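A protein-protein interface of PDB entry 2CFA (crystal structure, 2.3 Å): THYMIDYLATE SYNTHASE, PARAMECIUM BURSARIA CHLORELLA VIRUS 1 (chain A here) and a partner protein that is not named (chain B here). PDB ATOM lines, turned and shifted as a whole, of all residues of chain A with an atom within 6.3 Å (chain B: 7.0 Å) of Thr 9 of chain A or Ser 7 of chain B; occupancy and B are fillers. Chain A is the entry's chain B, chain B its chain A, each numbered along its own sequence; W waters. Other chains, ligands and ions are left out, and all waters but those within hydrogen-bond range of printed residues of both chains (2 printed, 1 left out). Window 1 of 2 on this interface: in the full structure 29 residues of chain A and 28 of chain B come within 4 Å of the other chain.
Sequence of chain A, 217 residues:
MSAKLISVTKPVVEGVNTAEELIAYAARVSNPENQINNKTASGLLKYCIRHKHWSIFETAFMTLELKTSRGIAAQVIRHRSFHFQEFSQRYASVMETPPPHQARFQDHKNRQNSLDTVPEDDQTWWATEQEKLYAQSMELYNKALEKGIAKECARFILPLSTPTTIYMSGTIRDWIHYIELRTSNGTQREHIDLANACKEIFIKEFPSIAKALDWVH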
ATOM      1  N   SER A   7      16.796  23.906  13.747  1.00  0.00           N
ATOM      2  CA  SER A   7      15.834  24.849  13.220  1.00  0.00           C
ATOM      3  C   SER A   7      14.489  24.197  13.003  1.00  0.00           C
ATOM      4  O   SER A   7      14.403  23.043  12.584  1.00  0.00           O
ATOM      5  CB  SER A   7      16.333  25.374  11.869  1.00  0.00           C
ATOM      6  OG  SER A   7      15.323  26.130  11.231  1.00  0.00           O
ATOM      7  N   VAL A   8      13.437  24.963  13.241  1.00  0.00           N
ATOM      8  CA  VAL A   8      12.089  24.504  12.974  1.00  0.00           C
ATOM      9  C   VAL A   8      11.164  25.683  12.666  1.00  0.00           C
ATOM     10  O   VAL A   8      11.387  26.816  13.107  1.00  0.00           O
ATOM     11  CB  VAL A   8      11.544  23.601  14.160  1.00  0.00           C
ATOM     12  CG1 VAL A   8      11.453  24.400  15.483  1.00  0.00           C
ATOM     13  CG2 VAL A   8      10.211  22.925  13.805  1.00  0.00           C
ATOM     14  N   THR A   9      10.153  25.382  11.857  1.00  0.00           N
ATOM     15  CA  THR A   9       8.987  26.211  11.574  1.00  0.00           C
ATOM     16  C   THR A   9       8.420  26.893  12.809  1.00  0.00           C
ATOM     17  O   THR A   9       8.049  26.212  13.783  1.00  0.00           O
ATOM     18  CB  THR A   9       7.878  25.306  10.946  1.00  0.00           C
ATOM     19  OG1 THR A   9       8.227  25.011   9.594  1.00  0.00           O
ATOM     20  CG2 THR A   9       6.510  25.977  10.952  1.00  0.00           C
ATOM     21  N   LYS A  10       8.353  28.229  12.763  1.00  0.00           N
ATOM     22  CA  LYS A  10       7.638  29.018  13.772  1.00  0.00           C
ATOM     23  C   LYS A  10       6.522  29.887  13.165  1.00  0.00           C
ATOM     24  O   LYS A  10       6.807  30.844  12.457  1.00  0.00           O
ATOM     25  CB  LYS A  10       8.622  29.875  14.581  1.00  0.00           C
ATOM     26  CG  LYS A  10       8.172  30.171  16.012  1.00  0.00           C
ATOM     27  CD  LYS A  10       9.401  30.218  16.946  1.00  0.00           C
ATOM     28  CE  LYS A  10       9.131  30.881  18.311  1.00  0.00           C
ATOM     29  NZ  LYS A  10      10.390  30.904  19.172  1.00  0.00           N
ATOM     30  N   PRO A  11       5.248  29.550  13.432  1.00  0.00           N
ATOM     31  CA  PRO A  11       4.146  30.387  12.922  1.00  0.00           C
ATOM     32  C   PRO A  11       4.111  31.809  13.495  1.00  0.00           C
ATOM     33  O   PRO A  11       4.674  32.077  14.561  1.00  0.00           O
ATOM     34  CB  PRO A  11       2.882  29.619  13.325  1.00  0.00           C
ATOM     35  CG  PRO A  11       3.314  28.683  14.376  1.00  0.00           C
ATOM     36  CD  PRO A  11       4.757  28.381  14.186  1.00  0.00           C
ATOM     37  N   VAL A  12       3.458  32.702  12.761  1.00  0.00           N
ATOM     38  CA  VAL A  12       3.323  34.106  13.136  1.00  0.00           C
ATOM     39  C   VAL A  12       1.857  34.534  13.091  1.00  0.00           C
ATOM     40  O   VAL A  12       1.548  35.721  13.238  1.00  0.00           O
ATOM     41  CB  VAL A  12       4.176  35.050  12.216  1.00  0.00           C
ATOM     42  CG1 VAL A  12       5.664  34.726  12.327  1.00  0.00           C
ATOM     43  CG2 VAL A  12       3.699  34.985  10.768  1.00  0.00           C
ATOM     44  N   VAL A  13       0.957  33.576  12.877  1.00  0.00           N
ATOM     45  CA  VAL A  13      -0.487  33.856  12.935  1.00  0.00           C
ATOM     46  C   VAL A  13      -0.925  33.944  14.414  1.00  0.00           C
ATOM     47  O   VAL A  13      -0.194  33.483  15.303  1.00  0.00           O
ATOM     48  CB  VAL A  13      -1.339  32.804  12.156  1.00  0.00           C
ATOM     49  CG1 VAL A  13      -0.561  32.179  11.010  1.00  0.00           C
ATOM     50  CG2 VAL A  13      -1.838  31.717  13.073  1.00  0.00           C
ATOM     51  N   ASN A  17       1.190  29.126  18.012  1.00  0.00           N
ATOM     52  CA  ASN A  17       2.469  29.459  18.602  1.00  0.00           C
ATOM     53  C   ASN A  17       3.604  28.568  18.121  1.00  0.00           C
ATOM     54  O   ASN A  17       4.729  29.038  17.954  1.00  0.00           O
ATOM     55  CB  ASN A  17       2.352  29.439  20.137  1.00  0.00           C
ATOM     56  CG  ASN A  17       1.238  30.354  20.646  1.00  0.00           C
ATOM     57  OD1 ASN A  17       0.121  29.906  20.909  1.00  0.00           O
ATOM     58  ND2 ASN A  17       1.527  31.645  20.740  1.00  0.00           N
ATOM     59  N   THR A  18       3.298  27.294  17.899  1.00  0.00           N
ATOM     60  CA  THR A  18       4.297  26.297  17.531  1.00  0.00           C
ATOM     61  C   THR A  18       4.008  25.687  16.163  1.00  0.00           C
ATOM     62  O   THR A  18       2.914  25.839  15.621  1.00  0.00           O
ATOM     63  CB  THR A  18       4.332  25.126  18.540  1.00  0.00           C
ATOM     64  OG1 THR A  18       3.082  24.417  18.491  1.00  0.00           O
ATOM     65  CG2 THR A  18       4.645  25.617  19.970  1.00  0.00           C
ATOM     66  N   ALA A  19       4.995  24.982  15.627  1.00  0.00           N
ATOM     67  CA  ALA A  19       4.821  24.198  14.400  1.00  0.00           C
ATOM     68  C   ALA A  19       3.671  23.188  14.528  1.00  0.00           C
ATOM     69  O   ALA A  19       2.839  23.066  13.630  1.00  0.00           O
ATOM     70  CB  ALA A  19       6.125  23.488  14.041  1.00  0.00           C
ATOM     71  N   GLU A  20       3.610  22.470  15.648  1.00  0.00           N
ATOM     72  CA  GLU A  20       2.553  21.461  15.823  1.00  0.00           C
ATOM     73  C   GLU A  20       1.154  22.076  15.808  1.00  0.00           C
ATOM     74  O   GLU A  20       0.217  21.495  15.255  1.00  0.00           O
ATOM     75  CB  GLU A  20       2.761  20.668  17.105  1.00  0.00           C
ATOM     76  CG  GLU A  20       1.737  19.574  17.277  1.00  0.00           C
ATOM     77  CD  GLU A  20       2.220  18.498  18.179  1.00  0.00           C
ATOM     78  OE1 GLU A  20       2.306  18.739  19.407  1.00  0.00           O
ATOM     79  OE2 GLU A  20       2.518  17.407  17.649  1.00  0.00           O
ATOM     80  N   LEU A  22       0.251  24.750  14.215  1.00  0.00           N
ATOM     81  CA  LEU A  22      -0.120  25.149  12.864  1.00  0.00           C
ATOM     82  C   LEU A  22      -0.679  23.968  12.080  1.00  0.00           C
ATOM     83  O   LEU A  22      -1.706  24.090  11.400  1.00  0.00           O
ATOM     84  CB  LEU A  22       1.062  25.827  12.136  1.00  0.00           C
ATOM     85  CG  LEU A  22       0.809  26.335  10.712  1.00  0.00           C
ATOM     86  CD1 LEU A  22      -0.349  27.339  10.627  1.00  0.00           C
ATOM     87  CD2 LEU A  22       2.070  26.951  10.172  1.00  0.00           C
ATOM     88  N   THR A  59       3.178  21.786   6.274  1.00  0.00           N
ATOM     89  CA  THR A  59       3.198  23.205   6.649  1.00  0.00           C
ATOM     90  C   THR A  59       4.363  23.502   7.599  1.00  0.00           C
ATOM     91  O   THR A  59       4.634  24.658   7.943  1.00  0.00           O
ATOM     92  CB  THR A  59       1.855  23.674   7.284  1.00  0.00           C
ATOM     93  OG1 THR A  59       1.466  22.795   8.350  1.00  0.00           O
ATOM     94  CG2 THR A  59       0.737  23.703   6.228  1.00  0.00           C
ATOM     95  N   ALA A  60       5.078  22.449   7.976  1.00  0.00           N
ATOM     96  CA  ALA A  60       6.114  22.530   8.982  1.00  0.00           C
ATOM     97  C   ALA A  60       7.348  21.829   8.455  1.00  0.00           C
ATOM     98  O   ALA A  60       7.259  20.850   7.723  1.00  0.00           O
ATOM     99  CB  ALA A  60       5.633  21.882  10.326  1.00  0.00           C
ATOM    100  N   PHE A  61       8.490  22.324   8.887  1.00  0.00           N
ATOM    101  CA  PHE A  61       9.788  21.976   8.347  1.00  0.00           C
ATOM    102  C   PHE A  61      10.675  22.043   9.550  1.00  0.00           C
ATOM    103  O   PHE A  61      10.535  22.952  10.389  1.00  0.00           O
ATOM    104  CB  PHE A  61      10.208  23.063   7.381  1.00  0.00           C
ATOM    105  CG  PHE A  61      11.311  22.697   6.444  1.00  0.00           C
ATOM    106  CD1 PHE A  61      12.586  23.216   6.623  1.00  0.00           C
ATOM    107  CD2 PHE A  61      11.062  21.921   5.320  1.00  0.00           C
ATOM    108  CE1 PHE A  61      13.597  22.943   5.721  1.00  0.00           C
ATOM    109  CE2 PHE A  61      12.082  21.634   4.401  1.00  0.00           C
ATOM    110  CZ  PHE A  61      13.339  22.150   4.594  1.00  0.00           C
ATOM    111  N   MET A  62      11.589  21.084   9.615  1.00  0.00           N
ATOM    112  CA  MET A  62      12.501  20.937  10.720  1.00  0.00           C
ATOM    113  C   MET A  62      13.834  20.559  10.130  1.00  0.00           C
ATOM    114  O   MET A  62      13.890  19.887   9.110  1.00  0.00           O
ATOM    115  CB  MET A  62      11.999  19.825  11.651  1.00  0.00           C
ATOM    116  CG  MET A  62      12.885  19.543  12.854  1.00  0.00           C
ATOM    117  SD  MET A  62      12.096  18.484  14.090  1.00  0.00           S
ATOM    118  CE  MET A  62      12.125  16.906  13.214  1.00  0.00           C
ATOM    119  N   PHE A 206       7.056  17.642  18.599  1.00  0.00           N
ATOM    120  CA  PHE A 206       5.703  17.297  18.163  1.00  0.00           C
ATOM    121  C   PHE A 206       5.086  16.220  19.069  1.00  0.00           C
ATOM    122  O   PHE A 206       4.758  15.132  18.587  1.00  0.00           O
ATOM    123  CB  PHE A 206       5.728  16.863  16.673  1.00  0.00           C
ATOM    124  CG  PHE A 206       6.302  17.915  15.753  1.00  0.00           C
ATOM    125  CD1 PHE A 206       7.651  17.901  15.418  1.00  0.00           C
ATOM    126  CD2 PHE A 206       5.502  18.946  15.269  1.00  0.00           C
ATOM    127  CE1 PHE A 206       8.191  18.885  14.603  1.00  0.00           C
ATOM    128  CE2 PHE A 206       6.033  19.939  14.447  1.00  0.00           C
ATOM    129  CZ  PHE A 206       7.379  19.911  14.111  1.00  0.00           C
ATOM    130  N   LYS B   4      -0.001  36.776   2.550  1.00  0.00           N
ATOM    131  CA  LYS B   4       0.244  37.042   3.952  1.00  0.00           C
ATOM    132  C   LYS B   4       1.208  35.976   4.439  1.00  0.00           C
ATOM    133  O   LYS B   4       1.064  34.804   4.077  1.00  0.00           O
ATOM    134  CB  LYS B   4      -1.081  36.962   4.717  1.00  0.00           C
ATOM    135  CG  LYS B   4      -0.990  37.275   6.198  1.00  0.00           C
ATOM    136  CD  LYS B   4      -2.207  36.759   6.959  1.00  0.00           C
ATOM    137  CE  LYS B   4      -1.934  36.690   8.466  1.00  0.00           C
ATOM    138  NZ  LYS B   4      -0.856  35.705   8.836  1.00  0.00           N
ATOM    139  N   LEU B   5       2.188  36.365   5.249  1.00  0.00           N
ATOM    140  CA  LEU B   5       3.090  35.395   5.857  1.00  0.00           C
ATOM    141  C   LEU B   5       2.368  34.596   6.961  1.00  0.00           C
ATOM    142  O   LEU B   5       1.690  35.172   7.809  1.00  0.00           O
ATOM    143  CB  LEU B   5       4.334  36.089   6.414  1.00  0.00           C
ATOM    144  CG  LEU B   5       5.339  35.268   7.235  1.00  0.00           C
ATOM    145  CD1 LEU B   5       6.285  34.488   6.334  1.00  0.00           C
ATOM    146  CD2 LEU B   5       6.121  36.185   8.128  1.00  0.00           C
ATOM    147  N   ILE B   6       2.508  33.272   6.923  1.00  0.00           N
ATOM    148  CA  ILE B   6       1.878  32.382   7.902  1.00  0.00           C
ATOM    149  C   ILE B   6       2.919  31.874   8.883  1.00  0.00           C
ATOM    150  O   ILE B   6       2.671  31.798  10.090  1.00  0.00           O
ATOM    151  CB  ILE B   6       1.138  31.190   7.196  1.00  0.00           C
ATOM    152  CG1 ILE B   6      -0.171  31.667   6.542  1.00  0.00           C
ATOM    153  CG2 ILE B   6       0.894  30.031   8.125  1.00  0.00           C
ATOM    154  CD1 ILE B   6      -1.132  32.475   7.452  1.00  0.00           C
ATOM    155  N   SER B   7       4.098  31.566   8.356  1.00  0.00           N
ATOM    156  CA  SER B   7       5.078  30.814   9.099  1.00  0.00           C
ATOM    157  C   SER B   7       6.409  30.794   8.387  1.00  0.00           C
ATOM    158  O   SER B   7       6.468  30.755   7.161  1.00  0.00           O
ATOM    159  CB  SER B   7       4.590  29.362   9.231  1.00  0.00           C
ATOM    160  OG  SER B   7       5.668  28.517   9.584  1.00  0.00           O
ATOM    161  N   VAL B   8       7.473  30.749   9.179  1.00  0.00           N
ATOM    162  CA  VAL B   8       8.823  30.725   8.663  1.00  0.00           C
ATOM    163  C   VAL B   8       9.744  29.965   9.628  1.00  0.00           C
ATOM    164  O   VAL B   8       9.504  29.917  10.837  1.00  0.00           O
ATOM    165  CB  VAL B   8       9.343  32.184   8.367  1.00  0.00           C
ATOM    166  CG1 VAL B   8       9.395  33.021   9.648  1.00  0.00           C
ATOM    167  CG2 VAL B   8      10.700  32.176   7.628  1.00  0.00           C
ATOM    168  N   THR B   9      10.770  29.352   9.058  1.00  0.00           N
ATOM    169  CA  THR B   9      11.925  28.778   9.760  1.00  0.00           C
ATOM    170  C   THR B   9      12.590  29.691  10.813  1.00  0.00           C
ATOM    171  O   THR B   9      13.049  30.796  10.510  1.00  0.00           O
ATOM    172  CB  THR B   9      12.976  28.347   8.680  1.00  0.00           C
ATOM    173  OG1 THR B   9      12.555  27.110   8.110  1.00  0.00           O
ATOM    174  CG2 THR B   9      14.397  28.176   9.241  1.00  0.00           C
ATOM    175  N   LYS B  10      12.665  29.213  12.048  1.00  0.00           N
ATOM    176  CA  LYS B  10      13.481  29.892  13.063  1.00  0.00           C
ATOM    177  C   LYS B  10      14.515  28.956  13.702  1.00  0.00           C
ATOM    178  O   LYS B  10      14.144  27.968  14.327  1.00  0.00           O
ATOM    179  CB  LYS B  10      12.605  30.541  14.142  1.00  0.00           C
ATOM    180  CG  LYS B  10      13.429  31.379  15.144  1.00  0.00           C
ATOM    181  CD  LYS B  10      12.568  32.074  16.166  1.00  0.00           C
ATOM    182  CE  LYS B  10      13.409  32.568  17.354  1.00  0.00           C
ATOM    183  NZ  LYS B  10      14.437  33.581  16.939  1.00  0.00           N
ATOM    184  N   PHE B  61      12.551  27.628   5.186  1.00  0.00           N
ATOM    185  CA  PHE B  61      11.273  27.206   4.649  1.00  0.00           C
ATOM    186  C   PHE B  61      10.271  28.233   5.139  1.00  0.00           C
ATOM    187  O   PHE B  61      10.329  28.651   6.298  1.00  0.00           O
ATOM    188  CB  PHE B  61      10.965  25.830   5.237  1.00  0.00           C
ATOM    189  CG  PHE B  61       9.791  25.104   4.628  1.00  0.00           C
ATOM    190  CD1 PHE B  61       8.528  25.166   5.220  1.00  0.00           C
ATOM    191  CD2 PHE B  61       9.966  24.254   3.531  1.00  0.00           C
ATOM    192  CE1 PHE B  61       7.455  24.419   4.705  1.00  0.00           C
ATOM    193  CE2 PHE B  61       8.882  23.515   3.004  1.00  0.00           C
ATOM    194  CZ  PHE B  61       7.641  23.600   3.596  1.00  0.00           C
ATOM    195  N   MET B  62       9.362  28.636   4.257  1.00  0.00           N
ATOM    196  CA  MET B  62       8.406  29.693   4.532  1.00  0.00           C
ATOM    197  C   MET B  62       7.050  29.336   3.944  1.00  0.00           C
ATOM    198  O   MET B  62       6.977  28.737   2.860  1.00  0.00           O
ATOM    199  CB  MET B  62       8.908  31.012   3.922  1.00  0.00           C
ATOM    200  CG  MET B  62       7.942  32.208   4.014  1.00  0.00           C
ATOM    201  SD  MET B  62       8.735  33.774   3.505  1.00  0.00           S
ATOM    202  CE  MET B  62       8.945  33.506   1.738  1.00  0.00           C
ATOM    203  N   THR B  63       5.989  29.702   4.667  1.00  0.00           N
ATOM    204  CA  THR B  63       4.615  29.504   4.234  1.00  0.00           C
ATOM    205  C   THR B  63       3.915  30.841   4.072  1.00  0.00           C
ATOM    206  O   THR B  63       4.010  31.715   4.934  1.00  0.00           O
ATOM    207  CB  THR B  63       3.815  28.620   5.242  1.00  0.00           C
ATOM    208  OG1 THR B  63       4.454  27.348   5.369  1.00  0.00           O
ATOM    209  CG2 THR B  63       2.381  28.404   4.777  1.00  0.00           C
ATOM    210  N   LEU B  64       3.207  30.989   2.958  1.00  0.00           N
ATOM    211  CA  LEU B  64       2.417  32.172   2.682  1.00  0.00           C
ATOM    212  C   LEU B  64       0.983  31.783   2.400  1.00  0.00           C
ATOM    213  O   LEU B  64       0.728  30.770   1.766  1.00  0.00           O
ATOM    214  CB  LEU B  64       2.983  32.926   1.473  1.00  0.00           C
ATOM    215  CG  LEU B  64       3.876  34.161   1.656  1.00  0.00           C
ATOM    216  CD1 LEU B  64       4.869  34.029   2.796  1.00  0.00           C
ATOM    217  CD2 LEU B  64       4.614  34.493   0.331  1.00  0.00           C
ATOM    218  N   GLU B  65       0.048  32.591   2.864  1.00  0.00           N
ATOM    219  CA  GLU B  65      -1.354  32.391   2.530  1.00  0.00           C
ATOM    220  C   GLU B  65      -1.683  33.276   1.342  1.00  0.00           C
ATOM    221  O   GLU B  65      -1.522  34.492   1.419  1.00  0.00           O
ATOM    222  CB  GLU B  65      -2.253  32.740   3.711  1.00  0.00           C
ATOM    223  CG  GLU B  65      -3.739  32.535   3.464  1.00  0.00           C
ATOM    224  CD  GLU B  65      -4.572  33.120   4.572  1.00  0.00           C
ATOM    225  OE1 GLU B  65      -4.689  34.364   4.623  1.00  0.00           O
ATOM    226  OE2 GLU B  65      -5.091  32.338   5.401  1.00  0.00           O
ATOM    227  N   MET B 168       0.960  28.093   0.635  1.00  0.00           N
ATOM    228  CA  MET B 168       2.029  27.714  -0.255  1.00  0.00           C
ATOM    229  C   MET B 168       3.286  27.716   0.590  1.00  0.00           C
ATOM    230  O   MET B 168       3.664  28.748   1.118  1.00  0.00           O
ATOM    231  CB  MET B 168       2.120  28.717  -1.422  1.00  0.00           C
ATOM    232  CG  MET B 168       3.178  28.419  -2.465  1.00  0.00           C
ATOM    233  SD  MET B 168       3.077  29.570  -3.870  1.00  0.00           S
ATOM    234  CE  MET B 168       4.538  29.158  -4.792  1.00  0.00           C
ATOM    235  N   SER B 169       3.923  26.555   0.700  1.00  0.00           N
ATOM    236  CA  SER B 169       5.080  26.349   1.560  1.00  0.00           C
ATOM    237  C   SER B 169       6.224  25.803   0.729  1.00  0.00           C
ATOM    238  O   SER B 169       6.046  24.855  -0.033  1.00  0.00           O
ATOM    239  CB  SER B 169       4.758  25.337   2.679  1.00  0.00           C
ATOM    240  OG  SER B 169       3.606  25.693   3.424  1.00  0.00           O
HETATM  241  O   HOH W   1       6.043  26.903   7.524  1.00  0.00           O
HETATM  242  O   HOH W   2       8.431  27.011   8.134  1.00  0.00           O
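Water W2 lies within hydrogen-bond range of the side-chain hydroxyl of Thr 9 of chain A (2.5 Å), the backbone carbonyl oxygen of Phe 61 of chain B (3.1 Å), the backbone NH of Thr 9 of chain B (3.4 Å) and the side-chain hydroxyl of Ser 7 of chain B (3.5 Å). Water W1 lies within hydrogen-bond range of OG of Ser 7 of chain B (2.6 Å), O of Thr 59 of chain A (2.7 Å) and OG1 of Thr 63 of chain B (2.7 Å).
Ser 7 of chain A touches Thr 9 of chain B. O of Val 8 of chain A touches C of Thr 9 of chain B, at 3.9 Å. C of Thr 9 of chain A touches O of Val 8 of chain B (3.8 Å). O of Lys 10 of chain A touches CA of Ser 7 of chain B, 3.8 Å away. CD of Lys 10 of chain B touches CD of Lys 10 of chain A, 3.8 Å away. Leu 5 of chain B touches Val 12 of chain A (O to CG2, 3.6 Å). CG1 of Val 13 of chain A touches O of Ile 6 of chain B, at 3.4 Å. CG2 of Ile 6 of chain B touches CD1 of Leu 22 of chain A (3.9 Å). Ser 7 of chain B touches Leu 22 of chain A. Phe 61 of chain A touches Phe 61 of chain B.
The backbone NH (N) of Lys 10 of chain B sits at hydrogen-bond distance from the backbone carbonyl oxygen (O) of Val 8 of chain A. The backbone NH (N) of Val 12 of chain A sits at hydrogen-bond distance from the backbone carbonyl oxygen (O) of Ile 6 of chain B (2.9 Å). The backbone carbonyl oxygen of Val 8 of chain B sits at hydrogen-bond distance from the backbone NH of Lys 10 of chain A, 2.8 Å away.
The side-chain hydroxyl (OG) of Ser 169 of chain B lies within hydrogen-bond range of the side-chain hydroxyl (OG1) of Thr 63 of chain B (2.7 Å). The backbone NH (N) of Thr 63 of chain B lies within hydrogen-bond range of the backbone carbonyl oxygen (O) of Ser 7 of chain B, 2.7 Å away. O of Phe 61 of chain B is in hydrogen-bond range of N of Thr 9 of chain B (2.9 Å). O of Thr 63 of chain B is in hydrogen-bond range of N of Ile 6 of chain B (2.9 Å). OG1 of Thr 9 of chain A is in hydrogen-bond range of N of Phe 61 of chain A (2.8 Å).
Thr 9 of chain A touches just these residues of chain B: Ser 7 (3.0 Å) and Val 8 (3.8 Å). Printed residues of chain B within 4 Å of Lys 10 of chain A: Ser 7, Val 8 and Lys 10. Ala 19 of chain A touches none of the printed residues of chain B. Printed residues of chain B within 4 Å of Phe 61 of chain A: Phe 61. Ser 7 of chain B touches just these residues of chain A: Thr 9 (3.0 Å), Lys 10 (3.8 Å), Pro 11 (3.9 Å) and Leu 22 (3.6 Å). Of the printed residues of chain A, Phe 61 of chain B touches Phe 61. The nearest residue of chain B that does not touch Thr 9 of chain A is Thr 9 of chain B (4.3 Å).
Hydrophobic or aromatic side chains of chain A that line the printed part of chain B: Pro 11, Val 12, Val 13, Leu 22 and Phe 61. Printed residues of chain B that touch a printed residue of chain A: Leu 5, Ile 6, Ser 7, Val 8, Thr 9, Lys 10, Phe 61 and Thr 63. Among the printed residues, 18 pairs touch across the chains. Among the printed residues, no Asp or Glu carboxylate lies within 4 Å of a Lys or Arg side-chain nitrogen of the other chain.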
